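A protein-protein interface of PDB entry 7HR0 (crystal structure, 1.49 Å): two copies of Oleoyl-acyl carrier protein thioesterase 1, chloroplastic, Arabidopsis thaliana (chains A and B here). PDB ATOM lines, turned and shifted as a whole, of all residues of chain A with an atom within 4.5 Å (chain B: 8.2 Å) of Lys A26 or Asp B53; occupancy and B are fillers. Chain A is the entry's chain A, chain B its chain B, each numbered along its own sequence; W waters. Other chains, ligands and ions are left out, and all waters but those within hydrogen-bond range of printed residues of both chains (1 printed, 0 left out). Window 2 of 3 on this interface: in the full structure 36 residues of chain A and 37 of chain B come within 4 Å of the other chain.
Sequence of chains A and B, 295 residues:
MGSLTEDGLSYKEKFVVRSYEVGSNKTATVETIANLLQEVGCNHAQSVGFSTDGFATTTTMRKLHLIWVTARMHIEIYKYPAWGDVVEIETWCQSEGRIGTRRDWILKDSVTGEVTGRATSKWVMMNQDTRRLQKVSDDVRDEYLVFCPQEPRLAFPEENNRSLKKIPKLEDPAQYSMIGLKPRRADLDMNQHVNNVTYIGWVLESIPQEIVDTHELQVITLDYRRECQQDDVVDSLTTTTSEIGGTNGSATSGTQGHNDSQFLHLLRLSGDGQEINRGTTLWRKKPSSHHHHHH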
ATOM      1  N   VAL A  22      21.747 -13.267  -9.836  1.00  0.00           N
ATOM      2  CA  VAL A  22      22.113 -14.517 -10.480  1.00  0.00           C
ATOM      3  C   VAL A  22      22.895 -14.321 -11.764  1.00  0.00           C
ATOM      4  O   VAL A  22      22.747 -13.301 -12.426  1.00  0.00           O
ATOM      5  CB  VAL A  22      20.883 -15.451 -10.714  1.00  0.00           C
ATOM      6  CG1 VAL A  22      20.057 -15.581  -9.440  1.00  0.00           C
ATOM      7  CG2 VAL A  22      20.023 -14.951 -11.852  1.00  0.00           C
ATOM      8  N   GLY A  23      23.698 -15.319 -12.102  1.00  0.00           N
ATOM      9  CA  GLY A  23      24.472 -15.317 -13.349  1.00  0.00           C
ATOM     10  C   GLY A  23      23.817 -16.133 -14.451  1.00  0.00           C
ATOM     11  O   GLY A  23      22.597 -16.325 -14.439  1.00  0.00           O
ATOM     12  N   SER A  24      24.632 -16.610 -15.404  1.00  0.00           N
ATOM     13  CA  SER A  24      24.218 -17.387 -16.576  1.00  0.00           C
ATOM     14  C   SER A  24      23.387 -18.632 -16.244  1.00  0.00           C
ATOM     15  O   SER A  24      22.402 -18.908 -16.926  1.00  0.00           O
ATOM     16  CB  SER A  24      25.432 -17.790 -17.417  1.00  0.00           C
ATOM     17  OG  SER A  24      26.530 -16.895 -17.309  1.00  0.00           O
ATOM     18  N   ASN A  25      23.759 -19.365 -15.182  1.00  0.00           N
ATOM     19  CA  ASN A  25      23.057 -20.593 -14.775  1.00  0.00           C
ATOM     20  C   ASN A  25      21.709 -20.315 -14.040  1.00  0.00           C
ATOM     21  O   ASN A  25      21.092 -21.251 -13.508  1.00  0.00           O
ATOM     22  CB  ASN A  25      23.956 -21.428 -13.845  1.00  0.00           C
ATOM     23  CG  ASN A  25      25.401 -21.585 -14.296  1.00  0.00           C
ATOM     24  OD1 ASN A  25      26.348 -21.062 -13.670  1.00  0.00           O
ATOM     25  ND2 ASN A  25      25.603 -22.311 -15.394  1.00  0.00           N
ATOM     26  N   LYS A  26      21.303 -19.027 -13.924  1.00  0.00           N
ATOM     27  CA  LYS A  26      20.153 -18.637 -13.125  1.00  0.00           C
ATOM     28  C   LYS A  26      20.375 -19.029 -11.662  1.00  0.00           C
ATOM     29  O   LYS A  26      19.409 -19.239 -10.943  1.00  0.00           O
ATOM     30  CB  LYS A  26      18.812 -19.187 -13.672  1.00  0.00           C
ATOM     31  CG  LYS A  26      18.431 -18.601 -15.025  1.00  0.00           C
ATOM     32  CD  LYS A  26      17.198 -19.283 -15.613  1.00  0.00           C
ATOM     33  CE  LYS A  26      17.092 -19.066 -17.108  1.00  0.00           C
ATOM     34  NZ  LYS A  26      16.199 -20.076 -17.752  1.00  0.00           N
ATOM     35  N   THR A  27      21.670 -19.087 -11.200  1.00  0.00           N
ATOM     36  CA  THR A  27      21.983 -19.315  -9.794  1.00  0.00           C
ATOM     37  C   THR A  27      22.861 -18.132  -9.297  1.00  0.00           C
ATOM     38  O   THR A  27      23.482 -17.437 -10.114  1.00  0.00           O
ATOM     39  CB  THR A  27      22.633 -20.685  -9.535  1.00  0.00           C
ATOM     40  OG1 THR A  27      23.923 -20.747 -10.138  1.00  0.00           O
ATOM     41  CG2 THR A  27      21.757 -21.850 -10.019  1.00  0.00           C
ATOM     42  N   ALA A  82      19.270 -20.917  -6.607  1.00  0.00           N
ATOM     43  CA  ALA A  82      18.660 -20.333  -7.777  1.00  0.00           C
ATOM     44  C   ALA A  82      17.836 -19.099  -7.402  1.00  0.00           C
ATOM     45  O   ALA A  82      17.495 -18.871  -6.237  1.00  0.00           O
ATOM     46  CB  ALA A  82      17.773 -21.382  -8.487  1.00  0.00           C
ATOM     47  N   TRP A  83      17.511 -18.287  -8.404  1.00  0.00           N
ATOM     48  CA  TRP A  83      16.649 -17.127  -8.287  1.00  0.00           C
ATOM     49  C   TRP A  83      15.304 -17.515  -7.584  1.00  0.00           C
ATOM     50  O   TRP A  83      14.657 -18.501  -7.987  1.00  0.00           O
ATOM     51  CB  TRP A  83      16.443 -16.702  -9.733  1.00  0.00           C
ATOM     52  CG  TRP A  83      15.442 -15.658 -10.014  1.00  0.00           C
ATOM     53  CD1 TRP A  83      14.955 -14.715  -9.163  1.00  0.00           C
ATOM     54  CD2 TRP A  83      14.874 -15.381 -11.296  1.00  0.00           C
ATOM     55  NE1 TRP A  83      14.036 -13.934  -9.810  1.00  0.00           N
ATOM     56  CE2 TRP A  83      13.971 -14.314 -11.128  1.00  0.00           C
ATOM     57  CE3 TRP A  83      14.989 -15.979 -12.556  1.00  0.00           C
ATOM     58  CZ2 TRP A  83      13.237 -13.783 -12.192  1.00  0.00           C
ATOM     59  CZ3 TRP A  83      14.252 -15.457 -13.610  1.00  0.00           C
ATOM     60  CH2 TRP A  83      13.408 -14.356 -13.429  1.00  0.00           C
ATOM     61  N   GLN B  46       6.643 -12.360 -12.790  1.00  0.00           N
ATOM     62  CA  GLN B  46       6.562 -13.803 -12.511  1.00  0.00           C
ATOM     63  C   GLN B  46       5.186 -14.193 -11.952  1.00  0.00           C
ATOM     64  O   GLN B  46       4.652 -15.288 -12.244  1.00  0.00           O
ATOM     65  CB  GLN B  46       7.625 -14.213 -11.492  1.00  0.00           C
ATOM     66  CG  GLN B  46       9.041 -14.165 -12.021  1.00  0.00           C
ATOM     67  CD  GLN B  46      10.000 -14.752 -11.008  1.00  0.00           C
ATOM     68  OE1 GLN B  46      10.458 -15.898 -11.134  1.00  0.00           O
ATOM     69  NE2 GLN B  46      10.294 -13.991  -9.956  1.00  0.00           N
ATOM     70  N   PHE B  50       4.559 -14.273 -16.722  1.00  0.00           N
ATOM     71  CA  PHE B  50       5.646 -13.999 -17.668  1.00  0.00           C
ATOM     72  C   PHE B  50       6.748 -15.054 -17.534  1.00  0.00           C
ATOM     73  O   PHE B  50       6.834 -15.736 -16.510  1.00  0.00           O
ATOM     74  CB  PHE B  50       6.224 -12.591 -17.467  1.00  0.00           C
ATOM     75  CG  PHE B  50       5.415 -11.463 -18.054  1.00  0.00           C
ATOM     76  CD1 PHE B  50       5.688 -10.980 -19.323  1.00  0.00           C
ATOM     77  CD2 PHE B  50       4.459 -10.812 -17.300  1.00  0.00           C
ATOM     78  CE1 PHE B  50       4.981  -9.900 -19.844  1.00  0.00           C
ATOM     79  CE2 PHE B  50       3.742  -9.748 -17.828  1.00  0.00           C
ATOM     80  CZ  PHE B  50       4.015  -9.292 -19.093  1.00  0.00           C
ATOM     81  N   SER B  51       7.603 -15.179 -18.567  1.00  0.00           N
ATOM     82  CA  SER B  51       8.709 -16.133 -18.575  1.00  0.00           C
ATOM     83  C   SER B  51       9.750 -15.831 -17.501  1.00  0.00           C
ATOM     84  O   SER B  51       9.931 -14.677 -17.119  1.00  0.00           O
ATOM     85  CB  SER B  51       9.383 -16.149 -19.942  1.00  0.00           C
ATOM     86  OG  SER B  51      10.112 -14.952 -20.162  1.00  0.00           O
ATOM     87  N   THR B  52      10.447 -16.869 -17.036  1.00  0.00           N
ATOM     88  CA  THR B  52      11.491 -16.735 -16.019  1.00  0.00           C
ATOM     89  C   THR B  52      12.864 -17.071 -16.622  1.00  0.00           C
ATOM     90  O   THR B  52      13.685 -17.719 -15.970  1.00  0.00           O
ATOM     91  CB  THR B  52      11.181 -17.647 -14.830  1.00  0.00           C
ATOM     92  OG1 THR B  52      11.244 -19.008 -15.277  1.00  0.00           O
ATOM     93  CG2 THR B  52       9.835 -17.342 -14.200  1.00  0.00           C
ATOM     94  N   ASP B  53      13.101 -16.667 -17.876  1.00  0.00           N
ATOM     95  CA  ASP B  53      14.384 -16.936 -18.522  1.00  0.00           C
ATOM     96  C   ASP B  53      15.253 -15.680 -18.710  1.00  0.00           C
ATOM     97  O   ASP B  53      16.202 -15.710 -19.490  1.00  0.00           O
ATOM     98  CB  ASP B  53      14.187 -17.692 -19.844  1.00  0.00           C
ATOM     99  CG  ASP B  53      13.708 -19.124 -19.640  1.00  0.00           C
ATOM    100  OD1 ASP B  53      12.529 -19.309 -19.254  1.00  0.00           O
ATOM    101  OD2 ASP B  53      14.513 -20.062 -19.870  1.00  0.00           O
ATOM    102  N   GLY B  54      14.960 -14.614 -17.964  1.00  0.00           N
ATOM    103  CA  GLY B  54      15.706 -13.364 -18.055  1.00  0.00           C
ATOM    104  C   GLY B  54      15.002 -12.309 -18.878  1.00  0.00           C
ATOM    105  O   GLY B  54      15.155 -11.110 -18.632  1.00  0.00           O
ATOM    106  N   PHE B  55      14.249 -12.750 -19.882  1.00  0.00           N
ATOM    107  CA  PHE B  55      13.462 -11.863 -20.715  1.00  0.00           C
ATOM    108  C   PHE B  55      12.032 -12.166 -20.335  1.00  0.00           C
ATOM    109  O   PHE B  55      11.528 -13.224 -20.710  1.00  0.00           O
ATOM    110  CB  PHE B  55      13.667 -12.187 -22.204  1.00  0.00           C
ATOM    111  CG  PHE B  55      15.084 -12.008 -22.691  1.00  0.00           C
ATOM    112  CD1 PHE B  55      15.602 -10.745 -22.912  1.00  0.00           C
ATOM    113  CD2 PHE B  55      15.891 -13.104 -22.943  1.00  0.00           C
ATOM    114  CE1 PHE B  55      16.902 -10.581 -23.370  1.00  0.00           C
ATOM    115  CE2 PHE B  55      17.195 -12.938 -23.387  1.00  0.00           C
ATOM    116  CZ  PHE B  55      17.692 -11.677 -23.600  1.00  0.00           C
ATOM    117  N   ALA B  56      11.385 -11.301 -19.555  1.00  0.00           N
ATOM    118  CA  ALA B  56       9.991 -11.512 -19.159  1.00  0.00           C
ATOM    119  C   ALA B  56       9.139 -11.328 -20.412  1.00  0.00           C
ATOM    120  O   ALA B  56       8.843 -10.207 -20.811  1.00  0.00           O
ATOM    121  CB  ALA B  56       9.592 -10.501 -18.100  1.00  0.00           C
ATOM    122  N   THR B  57       8.800 -12.433 -21.058  1.00  0.00           N
ATOM    123  CA  THR B  57       8.091 -12.418 -22.326  1.00  0.00           C
ATOM    124  C   THR B  57       6.731 -13.103 -22.219  1.00  0.00           C
ATOM    125  O   THR B  57       6.603 -14.063 -21.455  1.00  0.00           O
ATOM    126  CB  THR B  57       9.011 -13.133 -23.336  1.00  0.00           C
ATOM    127  OG1 THR B  57      10.127 -12.302 -23.630  1.00  0.00           O
ATOM    128  CG2 THR B  57       8.349 -13.441 -24.598  1.00  0.00           C
ATOM    129  N   ARG B  62       7.149 -14.788 -27.442  1.00  0.00           N
ATOM    130  CA  ARG B  62       8.091 -15.900 -27.630  1.00  0.00           C
ATOM    131  C   ARG B  62       7.979 -16.492 -29.036  1.00  0.00           C
ATOM    132  O   ARG B  62       8.993 -16.796 -29.659  1.00  0.00           O
ATOM    133  CB  ARG B  62       7.843 -17.013 -26.587  1.00  0.00           C
ATOM    134  CG  ARG B  62       8.519 -16.782 -25.249  1.00  0.00           C
ATOM    135  CD  ARG B  62       8.162 -17.875 -24.259  1.00  0.00           C
ATOM    136  NE  ARG B  62       9.358 -18.352 -23.568  1.00  0.00           N
ATOM    137  CZ  ARG B  62       9.344 -19.151 -22.503  1.00  0.00           C
ATOM    138  NH1 ARG B  62       8.192 -19.586 -22.002  1.00  0.00           N
ATOM    139  NH2 ARG B  62      10.483 -19.523 -21.929  1.00  0.00           N
ATOM    140  N   GLN B 128      14.172  -9.717 -31.055  1.00  0.00           N
ATOM    141  CA  GLN B 128      15.382 -10.155 -30.362  1.00  0.00           C
ATOM    142  C   GLN B 128      16.572 -10.488 -31.302  1.00  0.00           C
ATOM    143  O   GLN B 128      17.727 -10.283 -30.924  1.00  0.00           O
ATOM    144  CB  GLN B 128      15.033 -11.381 -29.523  1.00  0.00           C
ATOM    145  CG  GLN B 128      16.079 -11.783 -28.501  1.00  0.00           C
ATOM    146  CD  GLN B 128      15.578 -12.877 -27.578  1.00  0.00           C
ATOM    147  OE1 GLN B 128      14.533 -13.515 -27.805  1.00  0.00           O
ATOM    148  NE2 GLN B 128      16.329 -13.119 -26.510  1.00  0.00           N
ATOM    149  N   ASP B 189      23.604  -9.223 -16.524  1.00  0.00           N
ATOM    150  CA  ASP B 189      22.418  -9.944 -16.052  1.00  0.00           C
ATOM    151  C   ASP B 189      22.533 -11.437 -16.381  1.00  0.00           C
ATOM    152  O   ASP B 189      23.550 -11.875 -16.921  1.00  0.00           O
ATOM    153  CB  ASP B 189      21.128  -9.297 -16.605  1.00  0.00           C
ATOM    154  CG  ASP B 189      20.945  -9.321 -18.111  1.00  0.00           C
ATOM    155  OD1 ASP B 189      21.674 -10.071 -18.791  1.00  0.00           O
ATOM    156  OD2 ASP B 189      20.084  -8.564 -18.617  1.00  0.00           O
ATOM    157  N   MET B 190      21.480 -12.235 -16.074  1.00  0.00           N
ATOM    158  CA  MET B 190      21.505 -13.663 -16.350  1.00  0.00           C
ATOM    159  C   MET B 190      21.638 -13.996 -17.858  1.00  0.00           C
ATOM    160  O   MET B 190      22.087 -15.092 -18.211  1.00  0.00           O
ATOM    161  CB  MET B 190      20.287 -14.350 -15.708  1.00  0.00           C
ATOM    162  CG  MET B 190      18.948 -13.729 -16.097  1.00  0.00           C
ATOM    163  SD  MET B 190      17.543 -14.607 -15.323  1.00  0.00           S
ATOM    164  CE  MET B 190      17.248 -13.483 -13.850  1.00  0.00           C
ATOM    165  N   ASN B 191      21.349 -13.027 -18.749  1.00  0.00           N
ATOM    166  CA  ASN B 191      21.504 -13.252 -20.197  1.00  0.00           C
ATOM    167  C   ASN B 191      22.758 -12.618 -20.802  1.00  0.00           C
ATOM    168  O   ASN B 191      22.843 -12.472 -22.024  1.00  0.00           O
ATOM    169  CB  ASN B 191      20.267 -12.786 -20.950  1.00  0.00           C
ATOM    170  CG  ASN B 191      19.054 -13.557 -20.539  1.00  0.00           C
ATOM    171  OD1 ASN B 191      18.103 -12.998 -20.000  1.00  0.00           O
ATOM    172  ND2 ASN B 191      19.086 -14.866 -20.758  1.00  0.00           N
HETATM  173  O   HOH W   1      12.611 -11.603  -9.152  1.00  0.00           O
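OD2 of Asp B53 lies within salt-bridge range of NZ of Lys A26.
The backbone carbonyl oxygen of Lys A26 sits at hydrogen-bond distance from the backbone NH of Trp A83. OD1 of Asp B53 is in salt-bridge range of NH2 of Arg B62 (3.4 Å). The backbone carbonyl oxygen (O) of Asp B53 is in hydrogen-bond range of the side-chain amide nitrogen (ND2) of Asn B191, 3.3 Å away. N of Gly B54 lies close to SD of Met B190, 3.7 Å away.
CG2 of Val A22 touches CE of Met B190, 3.7 Å away. Gly A23 touches Met B190. Met B190 touches Ser A24 (O to CA, 3.5 Å). Lys A26 touches Thr B52 (CE to O, 3.8 Å). Gln B46 touches Trp A83. Trp A83 touches Thr B52. CE of Met B190 touches CZ3 of Trp A83, 3.6 Å away.
Of chain B, only Thr B52 (3.8 Å) and Asp B53 (2.7 Å) come within 4 Å of Lys A26. Of the printed residues of chain B, Trp A83 touches Gln B46 (3.6 Å), Thr B52 (3.3 Å) and Met B190 (3.6 Å). Printed residues of chain A within 4 Å of Thr B52: Lys A26 (3.8 Å) and Trp A83 (3.3 Å). Asp B53 touches one residue of chain A.
Printed residues of chain B that touch a printed residue of chain A: Gln B46, Thr B52, Asp B53 and Met B190. Hydrophobic or aromatic side chains of chain B that line the printed part of chain A: Met B190. Printed residues of chain A that touch a printed residue of chain B: Val A22, Gly A23, Ser A24, Lys A26 and Trp A83. Among the printed residues, Asp or Glu carboxylates within 4 Å of a Lys or Arg side-chain nitrogen of the other chain: Lys A26 with Asp B53 (2.7 Å).
No position is printed for both chains. Of the 8 pairs that touch across the chains among the printed residues, none has its exchanged pair printed and touching as well.
Water W1 bridges the indole nitrogen of Trp A83 (2.8 Å) and the side-chain amide nitrogen of Gln B46 (3.4 Å).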
